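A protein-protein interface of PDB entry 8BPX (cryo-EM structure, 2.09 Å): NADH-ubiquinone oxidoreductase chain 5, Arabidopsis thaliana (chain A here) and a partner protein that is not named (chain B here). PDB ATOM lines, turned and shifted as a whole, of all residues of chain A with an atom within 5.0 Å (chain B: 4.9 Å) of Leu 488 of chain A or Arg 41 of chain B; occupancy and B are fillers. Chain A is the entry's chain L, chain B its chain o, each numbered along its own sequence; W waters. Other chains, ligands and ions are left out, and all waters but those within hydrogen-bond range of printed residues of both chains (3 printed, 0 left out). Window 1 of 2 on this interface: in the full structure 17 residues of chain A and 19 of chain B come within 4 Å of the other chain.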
ATOM      1  N   ASP A 483      11.272 -23.930 -22.985  1.00  0.00           N
ATOM      2  CA  ASP A 483      10.863 -22.653 -22.344  1.00  0.00           C
ATOM      3  C   ASP A 483       9.469 -22.794 -21.779  1.00  0.00           C
ATOM      4  O   ASP A 483       9.292 -22.416 -20.664  1.00  0.00           O
ATOM      5  CB  ASP A 483      11.012 -21.445 -23.278  1.00  0.00           C
ATOM      6  CG  ASP A 483      10.733 -20.096 -22.660  1.00  0.00           C
ATOM      7  OD1 ASP A 483      11.521 -19.650 -21.833  1.00  0.00           O
ATOM      8  OD2 ASP A 483       9.737 -19.513 -23.044  1.00  0.00           O
ATOM      9  N   ILE A 486       9.843 -25.486 -18.534  1.00  0.00           N
ATOM     10  CA  ILE A 486      10.854 -25.294 -17.482  1.00  0.00           C
ATOM     11  C   ILE A 486      11.536 -23.941 -17.681  1.00  0.00           C
ATOM     12  O   ILE A 486      12.475 -23.687 -16.942  1.00  0.00           O
ATOM     13  CB  ILE A 486      11.862 -26.466 -17.482  1.00  0.00           C
ATOM     14  CG1 ILE A 486      12.683 -26.539 -18.774  1.00  0.00           C
ATOM     15  CG2 ILE A 486      11.213 -27.807 -17.138  1.00  0.00           C
ATOM     16  CD1 ILE A 486      13.917 -27.393 -18.681  1.00  0.00           C
ATOM     17  N   GLY A 487      11.142 -23.164 -18.691  1.00  0.00           N
ATOM     18  CA  GLY A 487      11.698 -21.793 -18.832  1.00  0.00           C
ATOM     19  C   GLY A 487      11.523 -21.010 -17.545  1.00  0.00           C
ATOM     20  O   GLY A 487      10.486 -21.057 -16.981  1.00  0.00           O
ATOM     21  N   LEU A 488      12.508 -20.240 -17.176  1.00  0.00           N
ATOM     22  CA  LEU A 488      12.545 -19.476 -15.935  1.00  0.00           C
ATOM     23  C   LEU A 488      11.302 -18.612 -15.770  1.00  0.00           C
ATOM     24  O   LEU A 488      11.027 -17.734 -16.591  1.00  0.00           O
ATOM     25  CB  LEU A 488      13.802 -18.604 -15.904  1.00  0.00           C
ATOM     26  CG  LEU A 488      14.568 -18.543 -14.584  1.00  0.00           C
ATOM     27  CD1 LEU A 488      15.031 -19.926 -14.173  1.00  0.00           C
ATOM     28  CD2 LEU A 488      15.743 -17.581 -14.674  1.00  0.00           C
ATOM     29  N   GLY A 489      10.554 -18.875 -14.702  1.00  0.00           N
ATOM     30  CA  GLY A 489       9.373 -18.112 -14.375  1.00  0.00           C
ATOM     31  C   GLY A 489       8.149 -18.411 -15.209  1.00  0.00           C
ATOM     32  O   GLY A 489       7.176 -17.655 -15.128  1.00  0.00           O
ATOM     33  N   THR A 490       8.157 -19.490 -15.990  1.00  0.00           N
ATOM     34  CA  THR A 490       7.037 -19.782 -16.878  1.00  0.00           C
ATOM     35  C   THR A 490       5.749 -19.980 -16.085  1.00  0.00           C
ATOM     36  O   THR A 490       5.756 -20.502 -14.969  1.00  0.00           O
ATOM     37  CB  THR A 490       7.337 -21.022 -17.734  1.00  0.00           C
ATOM     38  OG1 THR A 490       6.318 -21.189 -18.724  1.00  0.00           O
ATOM     39  CG2 THR A 490       7.426 -22.293 -16.885  1.00  0.00           C
ATOM     40  N   LEU A 506      15.954 -23.487  -9.480  1.00  0.00           N
ATOM     41  CA  LEU A 506      16.248 -23.477 -10.933  1.00  0.00           C
ATOM     42  C   LEU A 506      17.247 -22.337 -11.339  1.00  0.00           C
ATOM     43  O   LEU A 506      18.191 -22.669 -12.043  1.00  0.00           O
ATOM     44  CB  LEU A 506      14.972 -23.429 -11.732  1.00  0.00           C
ATOM     45  CG  LEU A 506      15.131 -23.579 -13.245  1.00  0.00           C
ATOM     46  CD1 LEU A 506      15.640 -24.961 -13.634  1.00  0.00           C
ATOM     47  CD2 LEU A 506      13.835 -23.256 -13.963  1.00  0.00           C
ATOM     48  N   ALA A 507      17.080 -21.104 -10.881  1.00  0.00           N
ATOM     49  CA  ALA A 507      18.009 -19.961 -11.159  1.00  0.00           C
ATOM     50  C   ALA A 507      19.431 -20.302 -10.737  1.00  0.00           C
ATOM     51  O   ALA A 507      20.271 -20.274 -11.592  1.00  0.00           O
ATOM     52  CB  ALA A 507      17.517 -18.710 -10.482  1.00  0.00           C
ATOM     53  N   GLU A 510      20.996 -22.749 -13.054  1.00  0.00           N
ATOM     54  CA  GLU A 510      21.426 -22.173 -14.324  1.00  0.00           C
ATOM     55  C   GLU A 510      22.509 -21.096 -14.162  1.00  0.00           C
ATOM     56  O   GLU A 510      23.130 -20.801 -15.143  1.00  0.00           O
ATOM     57  CB  GLU A 510      20.225 -21.684 -15.121  1.00  0.00           C
ATOM     58  CG  GLU A 510      19.566 -20.403 -14.734  1.00  0.00           C
ATOM     59  CD  GLU A 510      18.869 -19.906 -15.983  1.00  0.00           C
ATOM     60  OE1 GLU A 510      19.426 -20.073 -17.081  1.00  0.00           O
ATOM     61  OE2 GLU A 510      17.773 -19.368 -15.866  1.00  0.00           O
ATOM     62  N   PHE A 511      22.797 -20.641 -12.957  1.00  0.00           N
ATOM     63  CA  PHE A 511      23.642 -19.451 -12.890  1.00  0.00           C
ATOM     64  C   PHE A 511      24.820 -19.588 -11.929  1.00  0.00           C
ATOM     65  O   PHE A 511      25.888 -19.023 -12.178  1.00  0.00           O
ATOM     66  CB  PHE A 511      22.796 -18.232 -12.509  1.00  0.00           C
ATOM     67  CG  PHE A 511      21.876 -17.771 -13.602  1.00  0.00           C
ATOM     68  CD1 PHE A 511      22.289 -17.775 -14.921  1.00  0.00           C
ATOM     69  CD2 PHE A 511      20.589 -17.348 -13.311  1.00  0.00           C
ATOM     70  CE1 PHE A 511      21.440 -17.362 -15.928  1.00  0.00           C
ATOM     71  CE2 PHE A 511      19.736 -16.931 -14.314  1.00  0.00           C
ATOM     72  CZ  PHE A 511      20.162 -16.939 -15.623  1.00  0.00           C
ATOM     73  N   LEU B  34       9.100 -10.286 -15.064  1.00  0.00           N
ATOM     74  CA  LEU B  34       8.425 -11.540 -15.389  1.00  0.00           C
ATOM     75  C   LEU B  34       7.056 -11.289 -16.001  1.00  0.00           C
ATOM     76  O   LEU B  34       6.650 -11.998 -16.927  1.00  0.00           O
ATOM     77  CB  LEU B  34       8.302 -12.421 -14.142  1.00  0.00           C
ATOM     78  CG  LEU B  34       7.750 -13.839 -14.367  1.00  0.00           C
ATOM     79  CD1 LEU B  34       8.436 -14.546 -15.531  1.00  0.00           C
ATOM     80  CD2 LEU B  34       7.844 -14.674 -13.100  1.00  0.00           C
ATOM     81  N   LEU B  37       7.237 -10.646 -19.675  1.00  0.00           N
ATOM     82  CA  LEU B  37       7.758 -11.843 -20.319  1.00  0.00           C
ATOM     83  C   LEU B  37       6.685 -12.919 -20.427  1.00  0.00           C
ATOM     84  O   LEU B  37       6.543 -13.557 -21.473  1.00  0.00           O
ATOM     85  CB  LEU B  37       8.977 -12.368 -19.563  1.00  0.00           C
ATOM     86  CG  LEU B  37       9.413 -13.799 -19.897  1.00  0.00           C
ATOM     87  CD1 LEU B  37       9.912 -13.888 -21.330  1.00  0.00           C
ATOM     88  CD2 LEU B  37      10.476 -14.271 -18.938  1.00  0.00           C
ATOM     89  N   ASN B  38       5.901 -13.119 -19.365  1.00  0.00           N
ATOM     90  CA  ASN B  38       4.865 -14.146 -19.414  1.00  0.00           C
ATOM     91  C   ASN B  38       3.715 -13.738 -20.324  1.00  0.00           C
ATOM     92  O   ASN B  38       3.143 -14.592 -21.012  1.00  0.00           O
ATOM     93  CB  ASN B  38       4.360 -14.461 -18.007  1.00  0.00           C
ATOM     94  CG  ASN B  38       5.152 -15.567 -17.347  1.00  0.00           C
ATOM     95  OD1 ASN B  38       5.966 -16.222 -17.987  1.00  0.00           O
ATOM     96  ND2 ASN B  38       4.921 -15.779 -16.061  1.00  0.00           N
ATOM     97  N   LYS B  39       3.379 -12.443 -20.365  1.00  0.00           N
ATOM     98  CA  LYS B  39       2.400 -11.984 -21.346  1.00  0.00           C
ATOM     99  C   LYS B  39       2.845 -12.316 -22.767  1.00  0.00           C
ATOM    100  O   LYS B  39       2.072 -12.866 -23.565  1.00  0.00           O
ATOM    101  CB  LYS B  39       2.168 -10.484 -21.193  1.00  0.00           C
ATOM    102  CG  LYS B  39       0.842 -10.130 -20.573  1.00  0.00           C
ATOM    103  CD  LYS B  39       0.657  -8.634 -20.503  1.00  0.00           C
ATOM    104  CE  LYS B  39       1.214  -8.078 -19.210  1.00  0.00           C
ATOM    105  NZ  LYS B  39       0.589  -8.720 -18.024  1.00  0.00           N
ATOM    106  N   CYS B  40       4.104 -12.009 -23.097  1.00  0.00           N
ATOM    107  CA  CYS B  40       4.591 -12.317 -24.438  1.00  0.00           C
ATOM    108  C   CYS B  40       4.629 -13.821 -24.682  1.00  0.00           C
ATOM    109  O   CYS B  40       4.278 -14.284 -25.770  1.00  0.00           O
ATOM    110  CB  CYS B  40       5.976 -11.715 -24.671  1.00  0.00           C
ATOM    111  SG  CYS B  40       6.639 -12.124 -26.309  1.00  0.00           S
ATOM    112  N   ARG B  41       5.054 -14.594 -23.681  1.00  0.00           N
ATOM    113  CA  ARG B  41       5.153 -16.040 -23.848  1.00  0.00           C
ATOM    114  C   ARG B  41       3.793 -16.640 -24.163  1.00  0.00           C
ATOM    115  O   ARG B  41       3.672 -17.490 -25.054  1.00  0.00           O
ATOM    116  CB  ARG B  41       5.745 -16.673 -22.585  1.00  0.00           C
ATOM    117  CG  ARG B  41       7.264 -16.678 -22.554  1.00  0.00           C
ATOM    118  CD  ARG B  41       7.818 -17.755 -21.642  1.00  0.00           C
ATOM    119  NE  ARG B  41       7.857 -17.343 -20.248  1.00  0.00           N
ATOM    120  CZ  ARG B  41       8.912 -17.460 -19.451  1.00  0.00           C
ATOM    121  NH1 ARG B  41      10.051 -17.971 -19.881  1.00  0.00           N
ATOM    122  NH2 ARG B  41       8.815 -17.061 -18.186  1.00  0.00           N
ATOM    123  N   GLN B  42       2.754 -16.193 -23.456  1.00  0.00           N
ATOM    124  CA  GLN B  42       1.403 -16.662 -23.744  1.00  0.00           C
ATOM    125  C   GLN B  42       0.937 -16.217 -25.122  1.00  0.00           C
ATOM    126  O   GLN B  42       0.301 -16.992 -25.845  1.00  0.00           O
ATOM    127  CB  GLN B  42       0.440 -16.173 -22.667  1.00  0.00           C
ATOM    128  CG  GLN B  42       0.348 -17.086 -21.470  1.00  0.00           C
ATOM    129  CD  GLN B  42      -0.853 -16.768 -20.605  1.00  0.00           C
ATOM    130  OE1 GLN B  42      -1.297 -15.625 -20.527  1.00  0.00           O
ATOM    131  NE2 GLN B  42      -1.390 -17.791 -19.952  1.00  0.00           N
ATOM    132  N   ALA B  43       1.241 -14.976 -25.511  1.00  0.00           N
ATOM    133  CA  ALA B  43       0.791 -14.504 -26.818  1.00  0.00           C
ATOM    134  C   ALA B  43       1.487 -15.232 -27.965  1.00  0.00           C
ATOM    135  O   ALA B  43       0.916 -15.347 -29.053  1.00  0.00           O
ATOM    136  CB  ALA B  43       1.008 -12.997 -26.942  1.00  0.00           C
ATOM    137  N   GLU B  44       2.702 -15.734 -27.748  1.00  0.00           N
ATOM    138  CA  GLU B  44       3.483 -16.357 -28.812  1.00  0.00           C
ATOM    139  C   GLU B  44       3.519 -17.879 -28.728  1.00  0.00           C
ATOM    140  O   GLU B  44       4.398 -18.498 -29.335  1.00  0.00           O
ATOM    141  CB  GLU B  44       4.909 -15.812 -28.813  1.00  0.00           C
ATOM    142  CG  GLU B  44       4.992 -14.313 -28.725  1.00  0.00           C
ATOM    143  CD  GLU B  44       4.309 -13.654 -29.888  1.00  0.00           C
ATOM    144  OE1 GLU B  44       4.865 -13.692 -31.001  1.00  0.00           O
ATOM    145  OE2 GLU B  44       3.207 -13.107 -29.689  1.00  0.00           O
ATOM    146  N   PHE B  45       2.595 -18.494 -27.992  1.00  0.00           N
ATOM    147  CA  PHE B  45       2.516 -19.952 -27.866  1.00  0.00           C
ATOM    148  C   PHE B  45       3.801 -20.548 -27.288  1.00  0.00           C
ATOM    149  O   PHE B  45       4.152 -21.689 -27.588  1.00  0.00           O
ATOM    150  CB  PHE B  45       2.181 -20.614 -29.207  1.00  0.00           C
ATOM    151  CG  PHE B  45       0.884 -20.157 -29.810  1.00  0.00           C
ATOM    152  CD1 PHE B  45      -0.313 -20.761 -29.457  1.00  0.00           C
ATOM    153  CD2 PHE B  45       0.860 -19.133 -30.742  1.00  0.00           C
ATOM    154  CE1 PHE B  45      -1.504 -20.346 -30.012  1.00  0.00           C
ATOM    155  CE2 PHE B  45      -0.334 -18.712 -31.299  1.00  0.00           C
ATOM    156  CZ  PHE B  45      -1.516 -19.322 -30.936  1.00  0.00           C
ATOM    157  N   TYR B  46       4.510 -19.775 -26.466  1.00  0.00           N
ATOM    158  CA  TYR B  46       5.736 -20.214 -25.793  1.00  0.00           C
ATOM    159  C   TYR B  46       6.812 -20.692 -26.766  1.00  0.00           C
ATOM    160  O   TYR B  46       7.607 -21.571 -26.433  1.00  0.00           O
ATOM    161  CB  TYR B  46       5.454 -21.308 -24.756  1.00  0.00           C
ATOM    162  CG  TYR B  46       4.538 -20.903 -23.630  1.00  0.00           C
ATOM    163  CD1 TYR B  46       3.161 -20.953 -23.770  1.00  0.00           C
ATOM    164  CD2 TYR B  46       5.060 -20.452 -22.426  1.00  0.00           C
ATOM    165  CE1 TYR B  46       2.327 -20.574 -22.738  1.00  0.00           C
ATOM    166  CE2 TYR B  46       4.240 -20.076 -21.389  1.00  0.00           C
ATOM    167  CZ  TYR B  46       2.873 -20.137 -21.548  1.00  0.00           C
ATOM    168  OH  TYR B  46       2.058 -19.759 -20.507  1.00  0.00           O
ATOM    169  N   CYS B  51       9.894 -13.765 -28.054  1.00  0.00           N
ATOM    170  CA  CYS B  51      10.021 -13.144 -26.702  1.00  0.00           C
ATOM    171  C   CYS B  51      11.462 -13.018 -26.249  1.00  0.00           C
ATOM    172  O   CYS B  51      11.693 -12.815 -25.087  1.00  0.00           O
ATOM    173  CB  CYS B  51       9.164 -13.964 -25.699  1.00  0.00           C
ATOM    174  SG  CYS B  51       7.431 -14.079 -26.166  1.00  0.00           S
ATOM    175  N   ARG B  55      12.822 -12.152 -22.349  1.00  0.00           N
ATOM    176  CA  ARG B  55      13.460 -13.257 -21.643  1.00  0.00           C
ATOM    177  C   ARG B  55      14.883 -12.908 -21.233  1.00  0.00           C
ATOM    178  O   ARG B  55      15.304 -13.220 -20.116  1.00  0.00           O
ATOM    179  CB  ARG B  55      13.437 -14.511 -22.517  1.00  0.00           C
ATOM    180  CG  ARG B  55      13.981 -15.753 -21.853  1.00  0.00           C
ATOM    181  CD  ARG B  55      13.966 -16.929 -22.811  1.00  0.00           C
ATOM    182  NE  ARG B  55      12.615 -17.268 -23.237  1.00  0.00           N
ATOM    183  CZ  ARG B  55      12.169 -17.155 -24.478  1.00  0.00           C
ATOM    184  NH1 ARG B  55      12.929 -16.670 -25.445  1.00  0.00           N
ATOM    185  NH2 ARG B  55      10.925 -17.535 -24.757  1.00  0.00           N
ATOM    186  N   TYR B  58      14.775 -10.448 -18.238  1.00  0.00           N
ATOM    187  CA  TYR B  58      14.382 -11.145 -17.016  1.00  0.00           C
ATOM    188  C   TYR B  58      15.504 -12.039 -16.498  1.00  0.00           C
ATOM    189  O   TYR B  58      15.783 -12.068 -15.290  1.00  0.00           O
ATOM    190  CB  TYR B  58      13.111 -11.959 -17.266  1.00  0.00           C
ATOM    191  CG  TYR B  58      12.680 -12.792 -16.087  1.00  0.00           C
ATOM    192  CD1 TYR B  58      12.139 -12.199 -14.963  1.00  0.00           C
ATOM    193  CD2 TYR B  58      12.823 -14.174 -16.094  1.00  0.00           C
ATOM    194  CE1 TYR B  58      11.748 -12.951 -13.879  1.00  0.00           C
ATOM    195  CE2 TYR B  58      12.435 -14.939 -15.012  1.00  0.00           C
ATOM    196  CZ  TYR B  58      11.894 -14.319 -13.909  1.00  0.00           C
ATOM    197  OH  TYR B  58      11.502 -15.059 -12.825  1.00  0.00           O
ATOM    198  N   GLU B  59      16.164 -12.771 -17.394  1.00  0.00           N
ATOM    199  CA  GLU B  59      17.230 -13.670 -16.968  1.00  0.00           C
ATOM    200  C   GLU B  59      18.438 -12.902 -16.450  1.00  0.00           C
ATOM    201  O   GLU B  59      19.097 -13.351 -15.510  1.00  0.00           O
ATOM    202  CB  GLU B  59      17.624 -14.605 -18.110  1.00  0.00           C
ATOM    203  CG  GLU B  59      16.535 -15.595 -18.496  1.00  0.00           C
ATOM    204  CD  GLU B  59      16.846 -16.352 -19.768  1.00  0.00           C
ATOM    205  OE1 GLU B  59      16.119 -17.323 -20.064  1.00  0.00           O
ATOM    206  OE2 GLU B  59      17.811 -15.989 -20.470  1.00  0.00           O
ATOM    207  N   GLU B  62      17.555 -12.062 -12.891  1.00  0.00           N
ATOM    208  CA  GLU B  62      17.675 -13.223 -12.006  1.00  0.00           C
ATOM    209  C   GLU B  62      19.138 -13.580 -11.744  1.00  0.00           C
ATOM    210  O   GLU B  62      19.519 -13.915 -10.612  1.00  0.00           O
ATOM    211  CB  GLU B  62      16.927 -14.414 -12.602  1.00  0.00           C
ATOM    212  CG  GLU B  62      15.416 -14.255 -12.613  1.00  0.00           C
ATOM    213  CD  GLU B  62      14.787 -14.602 -11.278  1.00  0.00           C
ATOM    214  OE1 GLU B  62      15.246 -15.569 -10.640  1.00  0.00           O
ATOM    215  OE2 GLU B  62      13.846 -13.900 -10.863  1.00  0.00           O
HETATM  216  O   HOH W   1       9.389 -23.774 -25.533  1.00  0.00           O
HETATM  217  O   HOH W   2      13.891 -18.576 -19.136  1.00  0.00           O
HETATM  218  O   HOH W   3      11.414 -17.459 -11.623  1.00  0.00           O
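Water W3 bridges the side-chain hydroxyl (OH) of Tyr 58 of chain B (2.7 Å) and the backbone NH (N) of Gly 489 of chain A (3.5 Å). Water W2 bridges OE1 of Glu 59 of chain B (2.7 Å) and N of Leu 488 of chain A (2.9 Å). Water W1 bridges O of Tyr 46 of chain B (3.0 Å) and N of Asp 483 of chain A (3.2 Å).
Of the 16 printed residues of chain B, 8 touch a printed residue of chain A. Printed residues of chain B that touch a printed residue of chain A: Leu 34, Asn 38, Arg 41, Tyr 46, Arg 55, Tyr 58, Glu 59 and Glu 62. Hydrophobic or aromatic side chains of chain B that line the printed part of chain A: Leu 34, Tyr 46 and Tyr 58. Along chain B the printed residues that touch a printed residue of chain A span positions 34 to 62. Of the 10 printed residues of chain A, 6 touch a printed residue of chain B. Printed residues of chain A that touch a printed residue of chain B: Asp 483, Leu 488, Gly 489, Thr 490, Ala 507 and Phe 511.
Leu 488 of chain A touches Tyr 58 of chain B. CG of Glu 62 of chain B touches CD2 of Leu 488 of chain A, at 3.9 Å. Gly 489 of chain A touches Leu 34 of chain B (O to CD1, 3.4 Å). Arg 41 of chain B touches Gly 489 of chain A. Asn 38 of chain B touches Thr 490 of chain A. Tyr 46 of chain B touches Thr 490 of chain A. Glu 62 of chain B touches Ala 507 of chain A. Phe 511 of chain A touches Glu 59 of chain B (CZ to O, 3.7 Å).
Leu 488 of chain A touches just these residues of chain B: Arg 41, Tyr 58 and Glu 62. Of chain A, only Asp 483, Leu 488, Gly 489 and Thr 490 come within 4 Å of Arg 41 of chain B. Printed residues of chain B within 4 Å of Asp 483 of chain A: Arg 41 (3.0 Å) and Arg 55 (2.9 Å). Of the printed residues of chain A, Tyr 58 of chain B touches Leu 488 (3.5 Å). Of the printed residues of chain A, Tyr 46 of chain B touches Thr 490 (3.6 Å). Phe 45 of chain B touches none of the printed residues of chain A. Leu 37 of chain B touches none of the printed residues of chain A. The nearest printed residue of chain B that does not touch Leu 488 of chain A is Leu 37 of chain B (4.2 Å). The nearest residue of chain A that does not touch Arg 41 of chain B is Gly 487 of chain A (4.1 Å). The nearest printed residue of chain A that does not touch Arg 55 of chain B is Leu 488 of chain A (6.4 Å).
The guanidinium group (NH1) of Arg 41 of chain B is in salt-bridge range of the side-chain carboxylate (OD1) of Asp 483 of chain A, 3.0 Å away. The side-chain carboxylate of Asp 483 of chain A lies within salt-bridge range of the guanidinium group of Arg 55 of chain B (2.9 Å). NH2 of Arg 41 of chain B lies within hydrogen-bond range of O of Leu 488 of chain A (2.8 Å). The backbone carbonyl oxygen (O) of Gly 489 of chain A is in hydrogen-bond range of the side-chain amide nitrogen (ND2) of Asn 38 of chain B (3.1 Å). N of Thr 490 of chain A sits close to NH2 of Arg 41 of chain B, at 3.3 Å.
The side-chain amide oxygen of Asn 38 of chain B is in hydrogen-bond range of the guanidinium group of Arg 41 of chain B, at 3.0 Å. The backbone carbonyl oxygen (O) of Arg 41 of chain B lies within hydrogen-bond range of the backbone NH (N) of Tyr 46 of chain B. The backbone NH of Arg 41 of chain B is in hydrogen-bond range of the side-chain sulfur of Cys 51 of chain B, 3.5 Å away. OH of Tyr 58 of chain B is in hydrogen-bond range of OE2 of Glu 62 of chain B. SG of Cys 51 of chain B is disulfide-bonded to SG of Cys 40 of chain B.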
